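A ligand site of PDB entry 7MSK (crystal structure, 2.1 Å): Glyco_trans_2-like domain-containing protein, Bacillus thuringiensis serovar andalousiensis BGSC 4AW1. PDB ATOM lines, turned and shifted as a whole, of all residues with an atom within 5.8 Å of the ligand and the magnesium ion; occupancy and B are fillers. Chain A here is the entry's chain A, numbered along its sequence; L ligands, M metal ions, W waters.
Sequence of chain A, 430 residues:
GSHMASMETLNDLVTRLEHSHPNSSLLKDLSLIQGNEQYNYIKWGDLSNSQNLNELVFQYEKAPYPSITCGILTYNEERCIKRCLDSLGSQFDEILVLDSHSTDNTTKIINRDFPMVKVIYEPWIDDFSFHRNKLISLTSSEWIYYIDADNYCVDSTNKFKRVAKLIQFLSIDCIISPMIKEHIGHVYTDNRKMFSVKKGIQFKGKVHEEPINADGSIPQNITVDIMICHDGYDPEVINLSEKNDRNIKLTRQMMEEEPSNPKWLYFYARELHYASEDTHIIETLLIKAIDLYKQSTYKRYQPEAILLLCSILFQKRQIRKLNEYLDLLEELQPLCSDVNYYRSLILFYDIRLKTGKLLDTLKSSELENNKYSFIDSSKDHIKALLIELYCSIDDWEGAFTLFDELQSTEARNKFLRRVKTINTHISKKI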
ATOM      1  N   ILE A  72      -8.063  18.637  19.863  1.00  0.00           N
ATOM      2  CA  ILE A  72      -8.810  17.401  19.710  1.00  0.00           C
ATOM      3  C   ILE A  72      -8.746  16.628  21.021  1.00  0.00           C
ATOM      4  O   ILE A  72      -7.644  16.363  21.522  1.00  0.00           O
ATOM      5  CB  ILE A  72      -8.235  16.545  18.558  1.00  0.00           C
ATOM      6  CG1 ILE A  72      -8.203  17.315  17.236  1.00  0.00           C
ATOM      7  CG2 ILE A  72      -9.005  15.240  18.442  1.00  0.00           C
ATOM      8  CD1 ILE A  72      -7.429  16.653  16.137  1.00  0.00           C
ATOM      9  N   LEU A  73      -9.926  16.271  21.541  1.00  0.00           N
ATOM     10  CA  LEU A  73     -10.045  15.313  22.637  1.00  0.00           C
ATOM     11  C   LEU A  73     -10.069  13.908  22.041  1.00  0.00           C
ATOM     12  O   LEU A  73     -10.747  13.697  21.025  1.00  0.00           O
ATOM     13  CB  LEU A  73     -11.320  15.566  23.446  1.00  0.00           C
ATOM     14  CG  LEU A  73     -11.471  16.942  24.114  1.00  0.00           C
ATOM     15  CD1 LEU A  73     -12.816  17.031  24.820  1.00  0.00           C
ATOM     16  CD2 LEU A  73     -10.355  17.216  25.106  1.00  0.00           C
ATOM     17  N   THR A  74      -9.348  12.955  22.653  1.00  0.00           N
ATOM     18  CA  THR A  74      -9.420  11.557  22.239  1.00  0.00           C
ATOM     19  C   THR A  74      -9.559  10.614  23.439  1.00  0.00           C
ATOM     20  O   THR A  74      -8.948  10.807  24.491  1.00  0.00           O
ATOM     21  CB  THR A  74      -8.215  11.137  21.395  1.00  0.00           C
ATOM     22  OG1 THR A  74      -7.031  11.255  22.189  1.00  0.00           O
ATOM     23  CG2 THR A  74      -8.087  11.951  20.131  1.00  0.00           C
ATOM     24  N   TYR A  75     -10.416   9.611  23.263  1.00  0.00           N
ATOM     25  CA  TYR A  75     -10.462   8.433  24.096  1.00  0.00           C
ATOM     26  C   TYR A  75     -10.827   7.242  23.215  1.00  0.00           C
ATOM     27  O   TYR A  75     -11.959   7.157  22.757  1.00  0.00           O
ATOM     28  CB  TYR A  75     -11.455   8.644  25.251  1.00  0.00           C
ATOM     29  CG  TYR A  75     -11.513   7.519  26.240  1.00  0.00           C
ATOM     30  CD1 TYR A  75     -10.369   7.082  26.913  1.00  0.00           C
ATOM     31  CD2 TYR A  75     -12.722   6.903  26.556  1.00  0.00           C
ATOM     32  CE1 TYR A  75     -10.421   6.048  27.834  1.00  0.00           C
ATOM     33  CE2 TYR A  75     -12.790   5.884  27.477  1.00  0.00           C
ATOM     34  CZ  TYR A  75     -11.633   5.444  28.109  1.00  0.00           C
ATOM     35  OH  TYR A  75     -11.727   4.431  29.009  1.00  0.00           O
ATOM     36  N   ASN A  76      -9.846   6.387  22.898  1.00  0.00           N
ATOM     37  CA  ASN A  76     -10.043   5.127  22.193  1.00  0.00           C
ATOM     38  C   ASN A  76     -10.634   5.365  20.806  1.00  0.00           C
ATOM     39  O   ASN A  76     -11.671   4.819  20.452  1.00  0.00           O
ATOM     40  CB  ASN A  76     -10.874   4.147  23.019  1.00  0.00           C
ATOM     41  CG  ASN A  76     -10.136   3.734  24.280  1.00  0.00           C
ATOM     42  OD1 ASN A  76      -8.941   3.448  24.223  1.00  0.00           O
ATOM     43  ND2 ASN A  76     -10.804   3.777  25.422  1.00  0.00           N
ATOM     44  N   GLU A  77      -9.881   6.125  20.001  1.00  0.00           N
ATOM     45  CA  GLU A  77     -10.295   6.536  18.683  1.00  0.00           C
ATOM     46  C   GLU A  77      -9.371   5.934  17.611  1.00  0.00           C
ATOM     47  O   GLU A  77      -9.158   6.544  16.559  1.00  0.00           O
ATOM     48  CB  GLU A  77     -10.289   8.069  18.632  1.00  0.00           C
ATOM     49  CG  GLU A  77     -11.261   8.715  19.624  1.00  0.00           C
ATOM     50  CD  GLU A  77     -12.732   8.598  19.267  1.00  0.00           C
ATOM     51  OE1 GLU A  77     -13.053   7.944  18.250  1.00  0.00           O
ATOM     52  OE2 GLU A  77     -13.581   9.167  20.012  1.00  0.00           O
ATOM     53  N   LEU A  98      -5.524  16.141  23.371  1.00  0.00           N
ATOM     54  CA  LEU A  98      -5.626  15.792  24.783  1.00  0.00           C
ATOM     55  C   LEU A  98      -6.280  14.417  24.901  1.00  0.00           C
ATOM     56  O   LEU A  98      -7.464  14.265  24.629  1.00  0.00           O
ATOM     57  CB  LEU A  98      -6.449  16.873  25.508  1.00  0.00           C
ATOM     58  CG  LEU A  98      -6.557  16.738  27.026  1.00  0.00           C
ATOM     59  CD1 LEU A  98      -5.183  16.799  27.685  1.00  0.00           C
ATOM     60  CD2 LEU A  98      -7.471  17.812  27.587  1.00  0.00           C
ATOM     61  N   ASP A  99      -5.493  13.415  25.345  1.00  0.00           N
ATOM     62  CA  ASP A  99      -5.956  12.041  25.387  1.00  0.00           C
ATOM     63  C   ASP A  99      -6.255  11.651  26.833  1.00  0.00           C
ATOM     64  O   ASP A  99      -5.465  11.965  27.723  1.00  0.00           O
ATOM     65  CB  ASP A  99      -4.909  11.099  24.779  1.00  0.00           C
ATOM     66  CG  ASP A  99      -5.336   9.644  24.714  1.00  0.00           C
ATOM     67  OD1 ASP A  99      -6.008   9.286  23.724  1.00  0.00           O
ATOM     68  OD2 ASP A  99      -5.045   8.893  25.691  1.00  0.00           O
ATOM     69  N   SER A 100      -7.394  10.963  27.018  1.00  0.00           N
ATOM     70  CA  SER A 100      -7.847  10.491  28.330  1.00  0.00           C
ATOM     71  C   SER A 100      -7.287   9.103  28.649  1.00  0.00           C
ATOM     72  O   SER A 100      -8.036   8.267  29.148  1.00  0.00           O
ATOM     73  CB  SER A 100      -9.369  10.422  28.383  1.00  0.00           C
ATOM     74  OG  SER A 100      -9.984  11.660  28.071  1.00  0.00           O
ATOM     75  N   TRP A 124      -9.735  11.397  32.584  1.00  0.00           N
ATOM     76  CA  TRP A 124     -11.117  11.772  32.387  1.00  0.00           C
ATOM     77  C   TRP A 124     -11.798  11.954  33.743  1.00  0.00           C
ATOM     78  O   TRP A 124     -11.665  11.086  34.602  1.00  0.00           O
ATOM     79  CB  TRP A 124     -11.829  10.694  31.559  1.00  0.00           C
ATOM     80  CG  TRP A 124     -13.203  11.128  31.126  1.00  0.00           C
ATOM     81  CD1 TRP A 124     -14.403  10.646  31.542  1.00  0.00           C
ATOM     82  CD2 TRP A 124     -13.489  12.196  30.222  1.00  0.00           C
ATOM     83  NE1 TRP A 124     -15.424  11.331  30.959  1.00  0.00           N
ATOM     84  CE2 TRP A 124     -14.899  12.292  30.132  1.00  0.00           C
ATOM     85  CE3 TRP A 124     -12.700  13.075  29.466  1.00  0.00           C
ATOM     86  CZ2 TRP A 124     -15.526  13.237  29.316  1.00  0.00           C
ATOM     87  CZ3 TRP A 124     -13.319  14.002  28.664  1.00  0.00           C
ATOM     88  CH2 TRP A 124     -14.716  14.077  28.597  1.00  0.00           C
ATOM     89  N   PHE A 128     -16.588  17.476  30.180  1.00  0.00           N
ATOM     90  CA  PHE A 128     -16.086  17.881  28.873  1.00  0.00           C
ATOM     91  C   PHE A 128     -15.500  19.290  28.897  1.00  0.00           C
ATOM     92  O   PHE A 128     -14.521  19.544  28.180  1.00  0.00           O
ATOM     93  CB  PHE A 128     -17.173  17.782  27.802  1.00  0.00           C
ATOM     94  CG  PHE A 128     -17.304  16.402  27.216  1.00  0.00           C
ATOM     95  CD1 PHE A 128     -16.455  15.987  26.206  1.00  0.00           C
ATOM     96  CD2 PHE A 128     -18.257  15.511  27.691  1.00  0.00           C
ATOM     97  CE1 PHE A 128     -16.577  14.722  25.658  1.00  0.00           C
ATOM     98  CE2 PHE A 128     -18.356  14.229  27.173  1.00  0.00           C
ATOM     99  CZ  PHE A 128     -17.522  13.839  26.155  1.00  0.00           C
ATOM    100  N   HIS A 131     -11.893  19.356  30.271  1.00  0.00           N
ATOM    101  CA  HIS A 131     -11.007  18.868  29.237  1.00  0.00           C
ATOM    102  C   HIS A 131     -10.842  19.917  28.133  1.00  0.00           C
ATOM    103  O   HIS A 131      -9.706  20.195  27.759  1.00  0.00           O
ATOM    104  CB  HIS A 131     -11.430  17.471  28.778  1.00  0.00           C
ATOM    105  CG  HIS A 131     -10.803  16.427  29.636  1.00  0.00           C
ATOM    106  ND1 HIS A 131     -11.012  16.384  30.999  1.00  0.00           N
ATOM    107  CD2 HIS A 131      -9.880  15.467  29.351  1.00  0.00           C
ATOM    108  CE1 HIS A 131     -10.314  15.400  31.511  1.00  0.00           C
ATOM    109  NE2 HIS A 131      -9.591  14.833  30.541  1.00  0.00           N
ATOM    110  N   ARG A 132     -11.932  20.570  27.687  1.00  0.00           N
ATOM    111  CA  ARG A 132     -11.793  21.566  26.614  1.00  0.00           C
ATOM    112  C   ARG A 132     -11.050  22.815  27.090  1.00  0.00           C
ATOM    113  O   ARG A 132     -10.289  23.403  26.325  1.00  0.00           O
ATOM    114  CB  ARG A 132     -13.133  21.948  25.970  1.00  0.00           C
ATOM    115  CG  ARG A 132     -13.793  20.819  25.195  1.00  0.00           C
ATOM    116  CD  ARG A 132     -14.764  21.236  24.098  1.00  0.00           C
ATOM    117  NE  ARG A 132     -15.433  20.093  23.482  1.00  0.00           N
ATOM    118  CZ  ARG A 132     -14.882  19.271  22.577  1.00  0.00           C
ATOM    119  NH1 ARG A 132     -13.638  19.456  22.174  1.00  0.00           N
ATOM    120  NH2 ARG A 132     -15.566  18.246  22.090  1.00  0.00           N
ATOM    121  N   ILE A 147     -12.098  20.031  16.851  1.00  0.00           N
ATOM    122  CA  ILE A 147     -12.751  18.966  16.112  1.00  0.00           C
ATOM    123  C   ILE A 147     -12.667  17.693  16.951  1.00  0.00           C
ATOM    124  O   ILE A 147     -11.717  17.518  17.704  1.00  0.00           O
ATOM    125  CB  ILE A 147     -12.076  18.813  14.733  1.00  0.00           C
ATOM    126  CG1 ILE A 147     -12.909  17.942  13.789  1.00  0.00           C
ATOM    127  CG2 ILE A 147     -10.646  18.300  14.870  1.00  0.00           C
ATOM    128  CD1 ILE A 147     -12.466  18.015  12.351  1.00  0.00           C
ATOM    129  N   ASP A 148     -13.673  16.822  16.845  1.00  0.00           N
ATOM    130  CA  ASP A 148     -13.638  15.564  17.574  1.00  0.00           C
ATOM    131  C   ASP A 148     -13.059  14.483  16.654  1.00  0.00           C
ATOM    132  O   ASP A 148     -13.004  14.658  15.443  1.00  0.00           O
ATOM    133  CB  ASP A 148     -15.022  15.172  18.110  1.00  0.00           C
ATOM    134  CG  ASP A 148     -15.579  16.188  19.081  1.00  0.00           C
ATOM    135  OD1 ASP A 148     -14.773  16.858  19.767  1.00  0.00           O
ATOM    136  OD2 ASP A 148     -16.805  16.340  19.115  1.00  0.00           O
ATOM    137  N   ALA A 149     -12.645  13.366  17.261  1.00  0.00           N
ATOM    138  CA  ALA A 149     -11.863  12.347  16.549  1.00  0.00           C
ATOM    139  C   ALA A 149     -12.747  11.591  15.558  1.00  0.00           C
ATOM    140  O   ALA A 149     -12.228  11.074  14.558  1.00  0.00           O
ATOM    141  CB  ALA A 149     -11.196  11.425  17.522  1.00  0.00           C
ATOM    142  N   ASP A 150     -14.058  11.552  15.828  1.00  0.00           N
ATOM    143  CA  ASP A 150     -15.006  10.948  14.896  1.00  0.00           C
ATOM    144  C   ASP A 150     -15.547  11.972  13.904  1.00  0.00           C
ATOM    145  O   ASP A 150     -16.563  11.717  13.267  1.00  0.00           O
ATOM    146  CB  ASP A 150     -16.171  10.262  15.626  1.00  0.00           C
ATOM    147  CG  ASP A 150     -16.923  11.141  16.603  1.00  0.00           C
ATOM    148  OD1 ASP A 150     -16.606  12.347  16.661  1.00  0.00           O
ATOM    149  OD2 ASP A 150     -17.786  10.621  17.331  1.00  0.00           O
ATOM    150  N   ASN A 151     -14.848  13.096  13.743  1.00  0.00           N
ATOM    151  CA  ASN A 151     -15.195  14.101  12.747  1.00  0.00           C
ATOM    152  C   ASN A 151     -14.116  14.102  11.678  1.00  0.00           C
ATOM    153  O   ASN A 151     -12.983  13.711  11.973  1.00  0.00           O
ATOM    154  CB  ASN A 151     -15.232  15.517  13.330  1.00  0.00           C
ATOM    155  CG  ASN A 151     -16.361  15.794  14.293  1.00  0.00           C
ATOM    156  OD1 ASN A 151     -16.130  16.334  15.376  1.00  0.00           O
ATOM    157  ND2 ASN A 151     -17.597  15.515  13.898  1.00  0.00           N
ATOM    158  N   LYS A 193     -17.463  26.053  17.874  1.00  0.00           N
ATOM    159  CA  LYS A 193     -16.241  25.274  17.932  1.00  0.00           C
ATOM    160  C   LYS A 193     -14.979  26.109  17.753  1.00  0.00           C
ATOM    161  O   LYS A 193     -13.892  25.595  18.012  1.00  0.00           O
ATOM    162  CB  LYS A 193     -16.301  24.151  16.896  1.00  0.00           C
ATOM    163  CG  LYS A 193     -17.356  23.087  17.167  1.00  0.00           C
ATOM    164  CD  LYS A 193     -17.232  22.440  18.531  1.00  0.00           C
ATOM    165  CE  LYS A 193     -18.110  21.214  18.678  1.00  0.00           C
ATOM    166  NZ  LYS A 193     -17.731  20.456  19.896  1.00  0.00           N
ATOM    167  N   LYS A 206     -20.790  19.913  31.954  1.00  0.00           N
ATOM    168  CA  LYS A 206     -20.031  18.661  31.924  1.00  0.00           C
ATOM    169  C   LYS A 206     -20.295  17.880  30.655  1.00  0.00           C
ATOM    170  O   LYS A 206     -19.518  16.993  30.287  1.00  0.00           O
ATOM    171  CB  LYS A 206     -20.382  17.806  33.143  1.00  0.00           C
ATOM    172  CG  LYS A 206     -19.938  18.405  34.472  1.00  0.00           C
ATOM    173  CD  LYS A 206     -20.444  17.650  35.664  1.00  0.00           C
ATOM    174  CE  LYS A 206     -19.555  17.877  36.872  1.00  0.00           C
ATOM    175  NZ  LYS A 206     -19.982  17.010  37.997  1.00  0.00           N
ATOM    176  N   VAL A 207     -21.419  18.185  30.005  1.00  0.00           N
ATOM    177  CA  VAL A 207     -21.801  17.569  28.744  1.00  0.00           C
ATOM    178  C   VAL A 207     -22.698  18.579  28.024  1.00  0.00           C
ATOM    179  O   VAL A 207     -23.288  19.432  28.682  1.00  0.00           O
ATOM    180  CB  VAL A 207     -22.470  16.207  28.997  1.00  0.00           C
ATOM    181  CG1 VAL A 207     -23.860  16.336  29.608  1.00  0.00           C
ATOM    182  CG2 VAL A 207     -22.523  15.342  27.745  1.00  0.00           C
ATOM    183  N   HIS A 208     -22.784  18.492  26.692  1.00  0.00           N
ATOM    184  CA  HIS A 208     -23.489  19.490  25.892  1.00  0.00           C
ATOM    185  C   HIS A 208     -22.923  20.881  26.192  1.00  0.00           C
ATOM    186  O   HIS A 208     -23.665  21.866  26.289  1.00  0.00           O
ATOM    187  CB  HIS A 208     -25.002  19.466  26.179  1.00  0.00           C
ATOM    188  CG  HIS A 208     -25.572  18.086  26.075  1.00  0.00           C
ATOM    189  ND1 HIS A 208     -25.358  17.291  24.981  1.00  0.00           N
ATOM    190  CD2 HIS A 208     -26.288  17.354  26.939  1.00  0.00           C
ATOM    191  CE1 HIS A 208     -25.934  16.118  25.163  1.00  0.00           C
ATOM    192  NE2 HIS A 208     -26.501  16.134  26.354  1.00  0.00           N
ATOM    193  N   GLU A 209     -21.600  20.922  26.393  1.00  0.00           N
ATOM    194  CA  GLU A 209     -20.895  22.098  26.866  1.00  0.00           C
ATOM    195  C   GLU A 209     -20.885  23.191  25.811  1.00  0.00           C
ATOM    196  O   GLU A 209     -21.065  22.923  24.621  1.00  0.00           O
ATOM    197  CB  GLU A 209     -19.480  21.721  27.285  1.00  0.00           C
ATOM    198  CG  GLU A 209     -18.582  21.299  26.116  1.00  0.00           C
ATOM    199  CD  GLU A 209     -18.818  19.935  25.468  1.00  0.00           C
ATOM    200  OE1 GLU A 209     -19.693  19.177  25.967  1.00  0.00           O
ATOM    201  OE2 GLU A 209     -18.104  19.609  24.477  1.00  0.00           O
ATOM    202  N   HIS A 230     -19.527  13.705  10.596  1.00  0.00           N
ATOM    203  CA  HIS A 230     -19.567  13.058  11.899  1.00  0.00           C
ATOM    204  C   HIS A 230     -20.272  11.711  11.776  1.00  0.00           C
ATOM    205  O   HIS A 230     -21.376  11.676  11.273  1.00  0.00           O
ATOM    206  CB  HIS A 230     -20.326  13.921  12.909  1.00  0.00           C
ATOM    207  CG  HIS A 230     -20.304  13.402  14.309  1.00  0.00           C
ATOM    208  ND1 HIS A 230     -21.450  13.171  15.040  1.00  0.00           N
ATOM    209  CD2 HIS A 230     -19.278  13.051  15.116  1.00  0.00           C
ATOM    210  CE1 HIS A 230     -21.128  12.735  16.258  1.00  0.00           C
ATOM    211  NE2 HIS A 230     -19.801  12.639  16.318  1.00  0.00           N
ATOM    212  N   GLY A 232     -20.470   9.624  14.616  1.00  0.00           N
ATOM    213  CA  GLY A 232     -20.541   9.209  16.007  1.00  0.00           C
ATOM    214  C   GLY A 232     -21.950   8.830  16.490  1.00  0.00           C
ATOM    215  O   GLY A 232     -22.111   8.426  17.654  1.00  0.00           O
ATOM    216  N   TYR A 233     -22.954   8.959  15.613  1.00  0.00           N
ATOM    217  CA  TYR A 233     -24.291   8.457  15.882  1.00  0.00           C
ATOM    218  C   TYR A 233     -24.697   7.379  14.881  1.00  0.00           C
ATOM    219  O   TYR A 233     -25.874   7.043  14.772  1.00  0.00           O
ATOM    220  CB  TYR A 233     -25.320   9.595  15.914  1.00  0.00           C
ATOM    221  CG  TYR A 233     -24.969  10.749  16.825  1.00  0.00           C
ATOM    222  CD1 TYR A 233     -24.598  10.543  18.139  1.00  0.00           C
ATOM    223  CD2 TYR A 233     -25.014  12.057  16.363  1.00  0.00           C
ATOM    224  CE1 TYR A 233     -24.246  11.595  18.966  1.00  0.00           C
ATOM    225  CE2 TYR A 233     -24.697  13.125  17.187  1.00  0.00           C
ATOM    226  CZ  TYR A 233     -24.312  12.894  18.489  1.00  0.00           C
ATOM    227  OH  TYR A 233     -23.979  13.959  19.294  1.00  0.00           O
ATOM    228  N   LYS A 243     -23.305   5.559  24.643  1.00  0.00           N
ATOM    229  CA  LYS A 243     -23.176   7.011  24.548  1.00  0.00           C
ATOM    230  C   LYS A 243     -24.351   7.701  25.236  1.00  0.00           C
ATOM    231  O   LYS A 243     -24.200   8.742  25.857  1.00  0.00           O
ATOM    232  CB  LYS A 243     -23.178   7.480  23.091  1.00  0.00           C
ATOM    233  CG  LYS A 243     -21.888   8.072  22.573  1.00  0.00           C
ATOM    234  CD  LYS A 243     -22.164   8.911  21.330  1.00  0.00           C
ATOM    235  CE  LYS A 243     -20.918   9.502  20.708  1.00  0.00           C
ATOM    236  NZ  LYS A 243     -20.108   8.497  19.975  1.00  0.00           N
ATOM    237  N   ARG A 246     -23.902   7.537  28.949  1.00  0.00           N
ATOM    238  CA  ARG A 246     -22.885   8.510  29.350  1.00  0.00           C
ATOM    239  C   ARG A 246     -23.533   9.891  29.499  1.00  0.00           C
ATOM    240  O   ARG A 246     -23.291  10.571  30.501  1.00  0.00           O
ATOM    241  CB  ARG A 246     -21.720   8.499  28.352  1.00  0.00           C
ATOM    242  CG  ARG A 246     -20.657   9.551  28.628  1.00  0.00           C
ATOM    243  CD  ARG A 246     -19.895   9.979  27.378  1.00  0.00           C
ATOM    244  NE  ARG A 246     -20.704  10.691  26.389  1.00  0.00           N
ATOM    245  CZ  ARG A 246     -20.303  10.979  25.152  1.00  0.00           C
ATOM    246  NH1 ARG A 246     -19.120  10.585  24.721  1.00  0.00           N
ATOM    247  NH2 ARG A 246     -21.089  11.651  24.335  1.00  0.00           N
ATOM    248  N   ASN A 247     -24.380  10.285  28.543  1.00  0.00           N
ATOM    249  CA  ASN A 247     -24.912  11.643  28.520  1.00  0.00           C
ATOM    250  C   ASN A 247     -25.973  11.837  29.600  1.00  0.00           C
ATOM    251  O   ASN A 247     -26.042  12.902  30.203  1.00  0.00           O
ATOM    252  CB  ASN A 247     -25.461  12.014  27.128  1.00  0.00           C
ATOM    253  CG  ASN A 247     -24.433  12.079  26.009  1.00  0.00           C
ATOM    254  OD1 ASN A 247     -23.223  12.097  26.210  1.00  0.00           O
ATOM    255  ND2 ASN A 247     -24.922  12.157  24.781  1.00  0.00           N
HETATM  256  C1  LIG L   1     -21.172  15.415  21.047  1.00  0.00           C
HETATM  257  O1  LIG L   1     -20.302  14.390  20.599  1.00  0.00           O
HETATM  258  P1  LIG L   1     -20.475  12.795  20.709  1.00  0.00           P
HETATM  259  O2  LIG L   1     -21.684  12.398  21.480  1.00  0.00           O
HETATM  260  O3  LIG L   1     -20.209  12.202  19.363  1.00  0.00           O
HETATM  261  O4  LIG L   1     -19.214  12.484  21.646  1.00  0.00           O
HETATM  262  P2  LIG L   1     -17.814  11.792  21.238  1.00  0.00           P
HETATM  263  O5  LIG L   1     -17.501  12.175  19.841  1.00  0.00           O
HETATM  264  O6  LIG L   1     -17.960  10.375  21.634  1.00  0.00           O
HETATM  265  O7  LIG L   1     -16.852  12.578  22.258  1.00  0.00           O
HETATM  266  C2  LIG L   1     -16.363  13.909  21.899  1.00  0.00           C
HETATM  267  C3  LIG L   1     -14.858  13.847  21.841  1.00  0.00           C
HETATM  268  O8  LIG L   1     -14.338  13.665  23.185  1.00  0.00           O
HETATM  269  C4  LIG L   1     -13.507  12.518  23.230  1.00  0.00           C
HETATM  270  C5  LIG L   1     -13.879  11.639  22.041  1.00  0.00           C
HETATM  271  C6  LIG L   1     -14.291  12.693  20.998  1.00  0.00           C
HETATM  272  O9  LIG L   1     -13.244  13.151  20.158  1.00  0.00           O
HETATM  273  O10 LIG L   1     -12.749  10.896  21.619  1.00  0.00           O
HETATM  274  N1  LIG L   1     -13.697  11.852  24.540  1.00  0.00           N
HETATM  275  C7  LIG L   1     -12.643  11.867  25.433  1.00  0.00           C
HETATM  276  O11 LIG L   1     -11.565  12.379  25.194  1.00  0.00           O
HETATM  277  N2  LIG L   1     -12.885  11.232  26.628  1.00  0.00           N
HETATM  278  C8  LIG L   1     -14.062  10.625  27.022  1.00  0.00           C
HETATM  279  O12 LIG L   1     -14.106  10.090  28.131  1.00  0.00           O
HETATM  280  C9  LIG L   1     -15.112  10.638  26.056  1.00  0.00           C
HETATM  281  C10 LIG L   1     -14.902  11.247  24.869  1.00  0.00           C
HETATM  282  C11 LIG L   1     -20.661  16.688  20.447  1.00  0.00           C
HETATM  283  F1  LIG L   1     -20.645  16.585  19.041  1.00  0.00           F
HETATM  284  C12 LIG L   1     -19.254  16.890  20.969  1.00  0.00           C
HETATM  285  O13 LIG L   1     -18.611  17.968  20.312  1.00  0.00           O
HETATM  286  C13 LIG L   1     -19.377  17.143  22.463  1.00  0.00           C
HETATM  287  O14 LIG L   1     -18.115  17.429  22.996  1.00  0.00           O
HETATM  288  C14 LIG L   1     -19.948  15.873  23.104  1.00  0.00           C
HETATM  289  C15 LIG L   1     -20.219  16.025  24.582  1.00  0.00           C
HETATM  290  O15 LIG L   1     -20.866  17.256  24.905  1.00  0.00           O
HETATM  291  O16 LIG L   1     -21.197  15.500  22.463  1.00  0.00           O
HETATM  292 MG    MG M   1     -18.528  12.471  18.171  1.00  0.00          MG
HETATM  293  O   HOH W   1     -19.272  18.661  17.303  1.00  0.00           O
HETATM  294  O   HOH W   2      -9.491  13.569  26.576  1.00  0.00           O
HETATM  295  O   HOH W   3     -23.365  17.043  23.235  1.00  0.00           O
HETATM  296  O   HOH W   4     -19.597  16.237  16.103  1.00  0.00           O
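Water W2 lies within hydrogen-bond range of the side-chain hydroxyl of Ser 100, an oxygen (O11) of the ligand and the backbone carbonyl oxygen of Leu 98.
Water W3 lies within hydrogen-bond range of ND1 of His 208 (2.7 Å) and O16 of the ligand (2.8 Å).
The magnesium ion is bound by O5 of the ligand (2.0 Å), O3 of the ligand (2.1 Å), OD2 of Asp 150 (2.2 Å), NE2 of His 230 (2.3 Å) and OD1 of Asp 150 (2.4 Å).
The side-chain carboxylate (OE1) of Glu 209 lies within hydrogen-bond range of an oxygen (O15) of the ligand (2.5 Å).
OE2 of Glu 77 sits at hydrogen-bond distance from O10 of the ligand (2.5 Å).
The side-chain amino group of Lys 193 sits at hydrogen-bond distance from an oxygen (O13) of the ligand (2.7 Å).
O of Leu 73 lies within hydrogen-bond range of O9 of the ligand (2.7 Å).
An oxygen (O13) of the ligand lies within hydrogen-bond range of the side-chain carboxylate of Asp 148 (2.7 Å).
O14 of the ligand lies within hydrogen-bond range of NH2 of Arg 132 (2.8 Å).
An oxygen (O15) of the ligand is in hydrogen-bond range of the backbone NH (N) of His 208 (2.9 Å).
The backbone NH (N) of Ala 149 sits at hydrogen-bond distance from an oxygen (O9) of the ligand (3.0 Å).
NH2 of Arg 246 lies within salt-bridge range of O2 of the ligand (3.0 Å).
NE1 of Trp 124 lies close to O12 of the ligand.
The side-chain amino group (NZ) of Lys 243 is in salt-bridge range of an oxygen (O6) of the ligand (3.3 Å).
An oxygen (O10) of the ligand lies within hydrogen-bond range of the backbone NH (N) of Tyr 75 (3.1 Å).
The backbone NH (N) of Thr 74 lies close to an oxygen (O11) of the ligand (3.4 Å).
OG of Ser 100 lies within hydrogen-bond range of N2 of the ligand, 3.3 Å away.
The side-chain carboxylate (OE2) of Glu 209 is in salt-bridge range of the guanidinium group (NE) of Arg 132 (2.9 Å).
The backbone NH of Asp 148 is in hydrogen-bond range of the side-chain amide oxygen of Asn 151 (2.9 Å).
NH2 of Arg 246 lies within hydrogen-bond range of OD1 of Asn 247, 2.9 Å away.
The side-chain amino group (NZ) of Lys 243 sits at hydrogen-bond distance from the backbone carbonyl oxygen (O) of Gly 232 (3.1 Å).
The backbone carbonyl oxygen of Thr 74 is in hydrogen-bond range of the backbone NH of Ser 100 (3.0 Å).
The backbone NH (N) of Thr 74 sits at hydrogen-bond distance from the backbone carbonyl oxygen (O) of Leu 98 (3.0 Å).
OG1 of Thr 74 is in hydrogen-bond range of OD1 of Asp 99, at 2.7 Å.
N of Phe 128 is in hydrogen-bond range of O of Lys 206, at 3.0 Å.
Phe 128 touches the ligand.
CG2 of Val 207 touches O15 of the ligand, 3.8 Å away.
Tyr 233 touches the ligand (OH to O2, 3.5 Å).
Within 4 Å of the ligand: Leu 73, Thr 74, Tyr 75, Glu 77, Ser 100, Trp 124, Phe 128, Arg 132, Asp 148, Ala 149, Asp 150, Lys 193, Val 207, His 208, Glu 209, His 230, Tyr 233, Lys 243 and Arg 246.
Within 4 Å of the magnesium ion: Asp 150 and His 230.
The nearest printed residue that does not touch the magnesium ion is Asp 148 (4.3 Å).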
